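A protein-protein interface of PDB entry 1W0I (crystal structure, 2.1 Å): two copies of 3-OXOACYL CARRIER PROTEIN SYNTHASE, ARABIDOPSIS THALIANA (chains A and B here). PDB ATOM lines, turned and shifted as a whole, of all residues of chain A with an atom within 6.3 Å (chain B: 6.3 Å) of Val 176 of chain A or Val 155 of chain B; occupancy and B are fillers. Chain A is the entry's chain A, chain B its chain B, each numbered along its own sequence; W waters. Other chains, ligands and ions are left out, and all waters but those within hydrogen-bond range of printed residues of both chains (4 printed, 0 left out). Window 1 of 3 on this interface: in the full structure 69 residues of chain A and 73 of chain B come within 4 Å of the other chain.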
ATOM      1  N   GLY A 121      21.366  17.828  16.570  1.00  0.00           N
ATOM      2  CA  GLY A 121      22.203  18.529  15.620  1.00  0.00           C
ATOM      3  C   GLY A 121      23.560  18.920  16.162  1.00  0.00           C
ATOM      4  O   GLY A 121      23.778  18.968  17.374  1.00  0.00           O
ATOM      5  N   GLY A 122      24.482  19.178  15.243  1.00  0.00           N
ATOM      6  CA  GLY A 122      25.817  19.603  15.613  1.00  0.00           C
ATOM      7  C   GLY A 122      25.991  20.988  15.021  1.00  0.00           C
ATOM      8  O   GLY A 122      25.471  21.269  13.940  1.00  0.00           O
ATOM      9  N   GLY A 123      26.712  21.859  15.717  1.00  0.00           N
ATOM     10  CA  GLY A 123      26.902  23.210  15.221  1.00  0.00           C
ATOM     11  C   GLY A 123      27.952  23.387  14.138  1.00  0.00           C
ATOM     12  O   GLY A 123      27.701  24.062  13.137  1.00  0.00           O
ATOM     13  N   ILE A 124      29.122  22.780  14.333  1.00  0.00           N
ATOM     14  CA  ILE A 124      30.236  22.894  13.389  1.00  0.00           C
ATOM     15  C   ILE A 124      30.701  21.546  12.841  1.00  0.00           C
ATOM     16  O   ILE A 124      31.165  21.457  11.703  1.00  0.00           O
ATOM     17  CB  ILE A 124      31.450  23.577  14.055  1.00  0.00           C
ATOM     18  CG1 ILE A 124      30.989  24.800  14.849  1.00  0.00           C
ATOM     19  CG2 ILE A 124      32.454  23.994  12.997  1.00  0.00           C
ATOM     20  CD1 ILE A 124      32.114  25.511  15.573  1.00  0.00           C
ATOM     21  N   VAL A 155      27.470  17.260   9.799  1.00  0.00           N
ATOM     22  CA  VAL A 155      26.831  17.611  11.065  1.00  0.00           C
ATOM     23  C   VAL A 155      25.512  16.923  11.386  1.00  0.00           C
ATOM     24  O   VAL A 155      25.013  17.032  12.509  1.00  0.00           O
ATOM     25  CB  VAL A 155      26.628  19.139  11.181  1.00  0.00           C
ATOM     26  CG1 VAL A 155      27.971  19.843  11.084  1.00  0.00           C
ATOM     27  CG2 VAL A 155      25.685  19.633  10.101  1.00  0.00           C
ATOM     28  N   ASN A 156      24.945  16.212  10.418  1.00  0.00           N
ATOM     29  CA  ASN A 156      23.686  15.513  10.653  1.00  0.00           C
ATOM     30  C   ASN A 156      23.953  14.067  11.065  1.00  0.00           C
ATOM     31  O   ASN A 156      23.043  13.365  11.496  1.00  0.00           O
ATOM     32  CB  ASN A 156      22.817  15.525   9.388  1.00  0.00           C
ATOM     33  CG  ASN A 156      23.340  14.591   8.309  1.00  0.00           C
ATOM     34  OD1 ASN A 156      22.769  13.530   8.056  1.00  0.00           O
ATOM     35  ND2 ASN A 156      24.435  14.979   7.674  1.00  0.00           N
ATOM     36  N   ALA A 174      17.765  17.009  12.028  1.00  0.00           N
ATOM     37  CA  ALA A 174      18.821  17.782  12.653  1.00  0.00           C
ATOM     38  C   ALA A 174      18.608  19.253  12.343  1.00  0.00           C
ATOM     39  O   ALA A 174      18.350  19.633  11.200  1.00  0.00           O
ATOM     40  CB  ALA A 174      20.184  17.330  12.151  1.00  0.00           C
ATOM     41  N   ALA A 175      18.684  20.075  13.378  1.00  0.00           N
ATOM     42  CA  ALA A 175      18.544  21.504  13.201  1.00  0.00           C
ATOM     43  C   ALA A 175      19.921  22.078  13.482  1.00  0.00           C
ATOM     44  O   ALA A 175      20.580  21.687  14.449  1.00  0.00           O
ATOM     45  CB  ALA A 175      17.526  22.068  14.170  1.00  0.00           C
ATOM     46  N   VAL A 176      20.378  22.970  12.614  1.00  0.00           N
ATOM     47  CA  VAL A 176      21.677  23.596  12.807  1.00  0.00           C
ATOM     48  C   VAL A 176      21.463  25.094  12.812  1.00  0.00           C
ATOM     49  O   VAL A 176      21.093  25.693  11.800  1.00  0.00           O
ATOM     50  CB  VAL A 176      22.673  23.213  11.704  1.00  0.00           C
ATOM     51  CG1 VAL A 176      24.011  23.894  11.964  1.00  0.00           C
ATOM     52  CG2 VAL A 176      22.858  21.707  11.682  1.00  0.00           C
ATOM     53  N   THR A 177      21.689  25.692  13.974  1.00  0.00           N
ATOM     54  CA  THR A 177      21.492  27.116  14.146  1.00  0.00           C
ATOM     55  C   THR A 177      22.567  27.706  15.040  1.00  0.00           C
ATOM     56  O   THR A 177      22.274  28.428  15.991  1.00  0.00           O
ATOM     57  CB  THR A 177      20.102  27.391  14.745  1.00  0.00           C
ATOM     58  OG1 THR A 177      19.892  26.546  15.882  1.00  0.00           O
ATOM     59  CG2 THR A 177      19.013  27.095  13.710  1.00  0.00           C
ATOM     60  N   ALA A 178      23.821  27.389  14.720  1.00  0.00           N
ATOM     61  CA  ALA A 178      24.961  27.881  15.484  1.00  0.00           C
ATOM     62  C   ALA A 178      24.796  27.596  16.976  1.00  0.00           C
ATOM     63  O   ALA A 178      24.570  26.458  17.368  1.00  0.00           O
ATOM     64  CB  ALA A 178      25.145  29.388  15.242  1.00  0.00           C
ATOM     65  N   ALA A 180      22.410  28.067  18.859  1.00  0.00           N
ATOM     66  CA  ALA A 180      21.046  27.728  19.245  1.00  0.00           C
ATOM     67  C   ALA A 180      20.678  26.326  18.790  1.00  0.00           C
ATOM     68  O   ALA A 180      19.583  25.841  19.063  1.00  0.00           O
ATOM     69  CB  ALA A 180      20.069  28.738  18.649  1.00  0.00           C
ATOM     70  N   THR A 181      21.609  25.679  18.103  1.00  0.00           N
ATOM     71  CA  THR A 181      21.391  24.338  17.578  1.00  0.00           C
ATOM     72  C   THR A 181      20.681  23.373  18.531  1.00  0.00           C
ATOM     73  O   THR A 181      19.687  22.744  18.159  1.00  0.00           O
ATOM     74  CB  THR A 181      22.728  23.731  17.112  1.00  0.00           C
ATOM     75  OG1 THR A 181      23.237  24.511  16.023  1.00  0.00           O
ATOM     76  CG2 THR A 181      22.537  22.292  16.647  1.00  0.00           C
ATOM     77  N   HIS A 184      16.798  24.491  19.004  1.00  0.00           N
ATOM     78  CA  HIS A 184      15.973  24.229  17.826  1.00  0.00           C
ATOM     79  C   HIS A 184      15.827  22.736  17.540  1.00  0.00           C
ATOM     80  O   HIS A 184      14.799  22.304  17.025  1.00  0.00           O
ATOM     81  CB  HIS A 184      16.564  24.912  16.590  1.00  0.00           C
ATOM     82  CG  HIS A 184      16.434  26.402  16.597  1.00  0.00           C
ATOM     83  ND1 HIS A 184      15.257  27.051  16.289  1.00  0.00           N
ATOM     84  CD2 HIS A 184      17.337  27.373  16.868  1.00  0.00           C
ATOM     85  CE1 HIS A 184      15.442  28.356  16.368  1.00  0.00           C
ATOM     86  NE2 HIS A 184      16.696  28.579  16.718  1.00  0.00           N
ATOM     87  N   SER A 185      16.849  21.947  17.860  1.00  0.00           N
ATOM     88  CA  SER A 185      16.758  20.516  17.611  1.00  0.00           C
ATOM     89  C   SER A 185      15.674  19.907  18.509  1.00  0.00           C
ATOM     90  O   SER A 185      14.906  19.055  18.065  1.00  0.00           O
ATOM     91  CB  SER A 185      18.113  19.829  17.848  1.00  0.00           C
ATOM     92  OG  SER A 185      19.021  20.080  16.775  1.00  0.00           O
ATOM     93  N   PHE B  88      27.675  29.474  -0.991  1.00  0.00           N
ATOM     94  CA  PHE B  88      26.374  28.941  -0.609  1.00  0.00           C
ATOM     95  C   PHE B  88      25.462  30.020  -0.055  1.00  0.00           C
ATOM     96  O   PHE B  88      24.241  29.935  -0.180  1.00  0.00           O
ATOM     97  CB  PHE B  88      26.526  27.777   0.383  1.00  0.00           C
ATOM     98  CG  PHE B  88      26.884  28.192   1.781  1.00  0.00           C
ATOM     99  CD1 PHE B  88      25.895  28.380   2.744  1.00  0.00           C
ATOM    100  CD2 PHE B  88      28.214  28.373   2.142  1.00  0.00           C
ATOM    101  CE1 PHE B  88      26.227  28.743   4.055  1.00  0.00           C
ATOM    102  CE2 PHE B  88      28.560  28.736   3.447  1.00  0.00           C
ATOM    103  CZ  PHE B  88      27.563  28.921   4.405  1.00  0.00           C
ATOM    104  N   ILE B 120      16.528  28.140   5.523  1.00  0.00           N
ATOM    105  CA  ILE B 120      17.328  27.709   4.384  1.00  0.00           C
ATOM    106  C   ILE B 120      18.622  27.108   4.919  1.00  0.00           C
ATOM    107  O   ILE B 120      19.445  27.815   5.497  1.00  0.00           O
ATOM    108  CB  ILE B 120      17.700  28.895   3.476  1.00  0.00           C
ATOM    109  CG1 ILE B 120      16.432  29.612   3.004  1.00  0.00           C
ATOM    110  CG2 ILE B 120      18.525  28.391   2.292  1.00  0.00           C
ATOM    111  CD1 ILE B 120      16.694  30.968   2.336  1.00  0.00           C
ATOM    112  N   GLY B 121      18.806  25.810   4.728  1.00  0.00           N
ATOM    113  CA  GLY B 121      20.010  25.186   5.230  1.00  0.00           C
ATOM    114  C   GLY B 121      21.037  24.808   4.182  1.00  0.00           C
ATOM    115  O   GLY B 121      20.756  24.790   2.982  1.00  0.00           O
ATOM    116  N   GLY B 122      22.245  24.525   4.657  1.00  0.00           N
ATOM    117  CA  GLY B 122      23.329  24.110   3.790  1.00  0.00           C
ATOM    118  C   GLY B 122      23.764  22.743   4.281  1.00  0.00           C
ATOM    119  O   GLY B 122      23.734  22.480   5.485  1.00  0.00           O
ATOM    120  N   GLY B 123      24.164  21.867   3.366  1.00  0.00           N
ATOM    121  CA  GLY B 123      24.573  20.533   3.768  1.00  0.00           C
ATOM    122  C   GLY B 123      26.015  20.373   4.214  1.00  0.00           C
ATOM    123  O   GLY B 123      26.307  19.544   5.080  1.00  0.00           O
ATOM    124  N   ILE B 124      26.920  21.157   3.635  1.00  0.00           N
ATOM    125  CA  ILE B 124      28.339  21.060   3.975  1.00  0.00           C
ATOM    126  C   ILE B 124      28.951  22.391   4.385  1.00  0.00           C
ATOM    127  O   ILE B 124      29.766  22.450   5.304  1.00  0.00           O
ATOM    128  CB  ILE B 124      29.158  20.516   2.792  1.00  0.00           C
ATOM    129  CG1 ILE B 124      28.557  19.194   2.305  1.00  0.00           C
ATOM    130  CG2 ILE B 124      30.605  20.330   3.216  1.00  0.00           C
ATOM    131  CD1 ILE B 124      29.275  18.599   1.119  1.00  0.00           C
ATOM    132  N   GLY B 125      28.568  23.458   3.691  1.00  0.00           N
ATOM    133  CA  GLY B 125      29.100  24.767   4.015  1.00  0.00           C
ATOM    134  C   GLY B 125      30.184  25.231   3.065  1.00  0.00           C
ATOM    135  O   GLY B 125      29.984  25.269   1.850  1.00  0.00           O
ATOM    136  N   SER B 126      31.341  25.588   3.611  1.00  0.00           N
ATOM    137  CA  SER B 126      32.435  26.053   2.770  1.00  0.00           C
ATOM    138  C   SER B 126      33.748  25.368   3.105  1.00  0.00           C
ATOM    139  O   SER B 126      34.591  25.923   3.810  1.00  0.00           O
ATOM    140  CB  SER B 126      32.599  27.566   2.899  1.00  0.00           C
ATOM    141  OG  SER B 126      33.507  28.041   1.921  1.00  0.00           O
ATOM    142  N   LYS B 152      31.673  32.519   7.766  1.00  0.00           N
ATOM    143  CA  LYS B 152      31.650  31.952   6.425  1.00  0.00           C
ATOM    144  C   LYS B 152      31.456  30.446   6.378  1.00  0.00           C
ATOM    145  O   LYS B 152      30.996  29.910   5.372  1.00  0.00           O
ATOM    146  CB  LYS B 152      32.931  32.320   5.668  1.00  0.00           C
ATOM    147  CG  LYS B 152      32.917  33.726   5.101  1.00  0.00           C
ATOM    148  CD  LYS B 152      34.104  33.990   4.185  1.00  0.00           C
ATOM    149  CE  LYS B 152      35.410  34.096   4.962  1.00  0.00           C
ATOM    150  NZ  LYS B 152      36.538  34.584   4.107  1.00  0.00           N
ATOM    151  N   ILE B 153      31.784  29.758   7.466  1.00  0.00           N
ATOM    152  CA  ILE B 153      31.653  28.307   7.482  1.00  0.00           C
ATOM    153  C   ILE B 153      30.417  27.782   8.206  1.00  0.00           C
ATOM    154  O   ILE B 153      30.110  26.591   8.127  1.00  0.00           O
ATOM    155  CB  ILE B 153      32.903  27.649   8.099  1.00  0.00           C
ATOM    156  CG1 ILE B 153      33.065  28.084   9.554  1.00  0.00           C
ATOM    157  CG2 ILE B 153      34.135  28.046   7.305  1.00  0.00           C
ATOM    158  CD1 ILE B 153      34.218  27.405  10.248  1.00  0.00           C
ATOM    159  N   LEU B 154      29.713  28.662   8.914  1.00  0.00           N
ATOM    160  CA  LEU B 154      28.506  28.254   9.635  1.00  0.00           C
ATOM    161  C   LEU B 154      27.397  27.986   8.622  1.00  0.00           C
ATOM    162  O   LEU B 154      26.963  28.889   7.912  1.00  0.00           O
ATOM    163  CB  LEU B 154      28.077  29.347  10.620  1.00  0.00           C
ATOM    164  CG  LEU B 154      29.058  29.635  11.762  1.00  0.00           C
ATOM    165  CD1 LEU B 154      28.516  30.753  12.638  1.00  0.00           C
ATOM    166  CD2 LEU B 154      29.273  28.381  12.580  1.00  0.00           C
ATOM    167  N   VAL B 155      26.942  26.738   8.564  1.00  0.00           N
ATOM    168  CA  VAL B 155      25.911  26.339   7.611  1.00  0.00           C
ATOM    169  C   VAL B 155      24.528  26.946   7.818  1.00  0.00           C
ATOM    170  O   VAL B 155      23.617  26.666   7.043  1.00  0.00           O
ATOM    171  CB  VAL B 155      25.770  24.806   7.570  1.00  0.00           C
ATOM    172  CG1 VAL B 155      27.028  24.195   6.973  1.00  0.00           C
ATOM    173  CG2 VAL B 155      25.536  24.265   8.973  1.00  0.00           C
ATOM    174  N   ASN B 156      24.371  27.772   8.847  1.00  0.00           N
ATOM    175  CA  ASN B 156      23.089  28.410   9.131  1.00  0.00           C
ATOM    176  C   ASN B 156      23.091  29.881   8.729  1.00  0.00           C
ATOM    177  O   ASN B 156      22.071  30.557   8.833  1.00  0.00           O
ATOM    178  CB  ASN B 156      22.773  28.329  10.624  1.00  0.00           C
ATOM    179  CG  ASN B 156      23.755  29.129  11.469  1.00  0.00           C
ATOM    180  OD1 ASN B 156      24.961  28.869  11.451  1.00  0.00           O
ATOM    181  ND2 ASN B 156      23.243  30.110  12.207  1.00  0.00           N
ATOM    182  N   MET B 157      24.229  30.383   8.270  1.00  0.00           N
ATOM    183  CA  MET B 157      24.309  31.790   7.912  1.00  0.00           C
ATOM    184  C   MET B 157      23.456  32.215   6.730  1.00  0.00           C
ATOM    185  O   MET B 157      23.104  33.389   6.613  1.00  0.00           O
ATOM    186  CB  MET B 157      25.766  32.187   7.693  1.00  0.00           C
ATOM    187  CG  MET B 157      26.573  32.119   8.977  1.00  0.00           C
ATOM    188  SD  MET B 157      25.748  33.015  10.322  1.00  0.00           S
ATOM    189  CE  MET B 157      26.088  34.693   9.840  1.00  0.00           C
ATOM    190  N   ALA B 158      23.114  31.276   5.855  1.00  0.00           N
ATOM    191  CA  ALA B 158      22.282  31.620   4.713  1.00  0.00           C
ATOM    192  C   ALA B 158      20.956  32.194   5.217  1.00  0.00           C
ATOM    193  O   ALA B 158      20.513  33.238   4.744  1.00  0.00           O
ATOM    194  CB  ALA B 158      22.039  30.398   3.839  1.00  0.00           C
ATOM    195  N   SER B 159      20.332  31.535   6.191  1.00  0.00           N
ATOM    196  CA  SER B 159      19.067  32.047   6.701  1.00  0.00           C
ATOM    197  C   SER B 159      19.300  33.346   7.472  1.00  0.00           C
ATOM    198  O   SER B 159      18.423  34.207   7.532  1.00  0.00           O
ATOM    199  CB  SER B 159      18.362  31.007   7.587  1.00  0.00           C
ATOM    200  OG  SER B 159      19.082  30.759   8.777  1.00  0.00           O
ATOM    201  N   HIS B 173      15.683  29.651  11.274  1.00  0.00           N
ATOM    202  CA  HIS B 173      15.994  28.235  11.407  1.00  0.00           C
ATOM    203  C   HIS B 173      16.727  27.645  10.213  1.00  0.00           C
ATOM    204  O   HIS B 173      16.821  28.262   9.154  1.00  0.00           O
ATOM    205  CB  HIS B 173      14.640  27.535  11.631  1.00  0.00           C
ATOM    206  CG  HIS B 173      14.674  26.037  11.659  1.00  0.00           C
ATOM    207  ND1 HIS B 173      14.526  25.266  10.524  1.00  0.00           N
ATOM    208  CD2 HIS B 173      14.689  25.170  12.700  1.00  0.00           C
ATOM    209  CE1 HIS B 173      14.440  23.993  10.866  1.00  0.00           C
ATOM    210  NE2 HIS B 173      14.534  23.907  12.181  1.00  0.00           N
ATOM    211  N   ALA B 174      17.255  26.447  10.401  1.00  0.00           N
ATOM    212  CA  ALA B 174      17.939  25.743   9.336  1.00  0.00           C
ATOM    213  C   ALA B 174      17.930  24.273   9.696  1.00  0.00           C
ATOM    214  O   ALA B 174      18.187  23.896  10.843  1.00  0.00           O
ATOM    215  CB  ALA B 174      19.372  26.247   9.183  1.00  0.00           C
ATOM    216  N   ALA B 175      17.580  23.450   8.719  1.00  0.00           N
ATOM    217  CA  ALA B 175      17.569  22.012   8.913  1.00  0.00           C
ATOM    218  C   ALA B 175      18.738  21.499   8.083  1.00  0.00           C
ATOM    219  O   ALA B 175      18.883  21.870   6.917  1.00  0.00           O
ATOM    220  CB  ALA B 175      16.251  21.410   8.415  1.00  0.00           C
ATOM    221  N   VAL B 176      19.587  20.679   8.691  1.00  0.00           N
ATOM    222  CA  VAL B 176      20.735  20.115   7.993  1.00  0.00           C
ATOM    223  C   VAL B 176      20.686  18.600   8.101  1.00  0.00           C
ATOM    224  O   VAL B 176      20.920  18.015   9.165  1.00  0.00           O
ATOM    225  CB  VAL B 176      22.074  20.624   8.567  1.00  0.00           C
ATOM    226  CG1 VAL B 176      23.234  20.004   7.800  1.00  0.00           C
ATOM    227  CG2 VAL B 176      22.137  22.141   8.453  1.00  0.00           C
ATOM    228  N   THR B 206      20.717  25.280  -0.016  1.00  0.00           N
ATOM    229  CA  THR B 206      21.782  25.819  -0.828  1.00  0.00           C
ATOM    230  C   THR B 206      23.057  25.009  -0.650  1.00  0.00           C
ATOM    231  O   THR B 206      23.297  24.422   0.406  1.00  0.00           O
ATOM    232  CB  THR B 206      22.064  27.278  -0.450  1.00  0.00           C
ATOM    233  OG1 THR B 206      23.065  27.811  -1.328  1.00  0.00           O
ATOM    234  CG2 THR B 206      22.560  27.360   1.000  1.00  0.00           C
HETATM  235  O   HOH W   1      24.549  17.365   6.524  1.00  0.00           O
HETATM  236  O   HOH W   2      28.221  24.943  10.347  1.00  0.00           O
HETATM  237  O   HOH W   3      27.797  19.162   7.526  1.00  0.00           O
HETATM  238  O   HOH W   4      25.637  26.323  12.508  1.00  0.00           O
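OG of Ser 159 of chain B lies within hydrogen-bond range of O of Asn 156 of chain B, 3.0 Å away.
The backbone carbonyl oxygen (O) of Ala 175 of chain A lies within hydrogen-bond range of the side-chain hydroxyl (OG) of Ser 185 of chain A (3.2 Å).
N of Thr 177 of chain A is in hydrogen-bond range of OG1 of Thr 181 of chain A (2.8 Å).
The backbone carbonyl oxygen of Ala 178 of chain A is in hydrogen-bond range of the side-chain hydroxyl of Thr 181 of chain A.
The side-chain hydroxyl (OG) of Ser 159 of chain B sits at hydrogen-bond distance from the backbone carbonyl oxygen (O) of His 173 of chain B (3.4 Å).
N of Gly 122 of chain B is in hydrogen-bond range of O of Val 155 of chain B, at 3.5 Å.
Water W1 lies within hydrogen-bond range of ND2 of Asn 156 of chain A (2.7 Å) and O of Gly 123 of chain B (3.2 Å).
Water W2 lies within hydrogen-bond range of the backbone NH (N) of Val 155 of chain B (2.8 Å), the backbone carbonyl oxygen (O) of Gly 123 of chain A (3.0 Å) and the backbone carbonyl oxygen (O) of Ile 153 of chain B (3.3 Å).
Water W4 lies within hydrogen-bond range of OD1 of Asn 156 of chain B (2.8 Å), N of Ala 178 of chain A (3.1 Å) and O of Gly 123 of chain A (3.1 Å).
Water W3 lies within hydrogen-bond range of the backbone carbonyl oxygen (O) of Gly 123 of chain B (2.9 Å) and the backbone NH (N) of Val 155 of chain A (3.0 Å).
Printed residues of chain B within 4 Å of Val 155 of chain A: Val 176.
Printed residues of chain B within 4 Å of Asn 156 of chain A: Val 176.
Ser 126 of chain B touches none of the printed residues of chain A.
Ile 153 of chain B touches none of the printed residues of chain A.
Val 155 of chain B touches just one residue of chain A: Val 176.
Printed residues of chain A within 4 Å of Val 176 of chain B: Val 155, Asn 156, Ala 174 and Val 176.
The nearest residue of chain B that does not touch Val 176 of chain A is Ala 175 of chain B (4.7 Å).
Hydrophobic or aromatic side chains of chain A within 4 Å of the printed part of chain B: Val 155, Ala 174, Ala 175, Val 176 and Ala 178.
Of the 21 printed residues of chain B, 6 touch a printed residue of chain A.
Hydrophobic or aromatic side chains of chain B within 4 Å of the printed part of chain A: Val 155, Ala 174, Ala 175 and Val 176.
Among the printed residues, 13 pairs touch across the chains.
Among the printed residues, merely in contact across the chains: Asn 156 of chain A with Val 176 of chain B, Val 176 of chain A with Val 176 of chain B, Val 176 of chain A with Asn 156 of chain B, Ala 175 of chain A with Ala 174 of chain B, Val 176 of chain A with Val 155 of chain B, Val 155 of chain A with Val 176 of chain B, Ala 174 of chain A with Ala 175 of chain B, Ala 178 of chain A with Asn 156 of chain B, Thr 177 of chain A with Asn 156 of chain B, Thr 177 of chain A with Ala 174 of chain B and Thr 177 of chain A with His 173 of chain B.
O of Ala 174 of chain A lies within hydrogen-bond range of N of Val 176 of chain B (3.0 Å).
N of Val 176 of chain A lies within hydrogen-bond range of O of Ala 174 of chain B, at 3.0 Å.
Val 155 of chain A touches Val 176 of chain B, and with the chains exchanged Val 176 of chain A touches Val 155 of chain B.
Asn 156 of chain A touches Val 176 of chain B, and with the chains exchanged Val 176 of chain A touches Asn 156 of chain B.
Ala 174 of chain A touches Val 176 of chain B, and with the chains exchanged Val 176 of chain A touches Ala 174 of chain B.
Val 176 of chain B touches its own counterpart, Val 176 of chain A.
Positions printed for both chains: 121, 122, 123, 124, 155, 156, 174, 175 and 176.
Of the 13 pairs that touch across the chains among the printed residues, 9 have their exchanged pair printed and touching as well.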
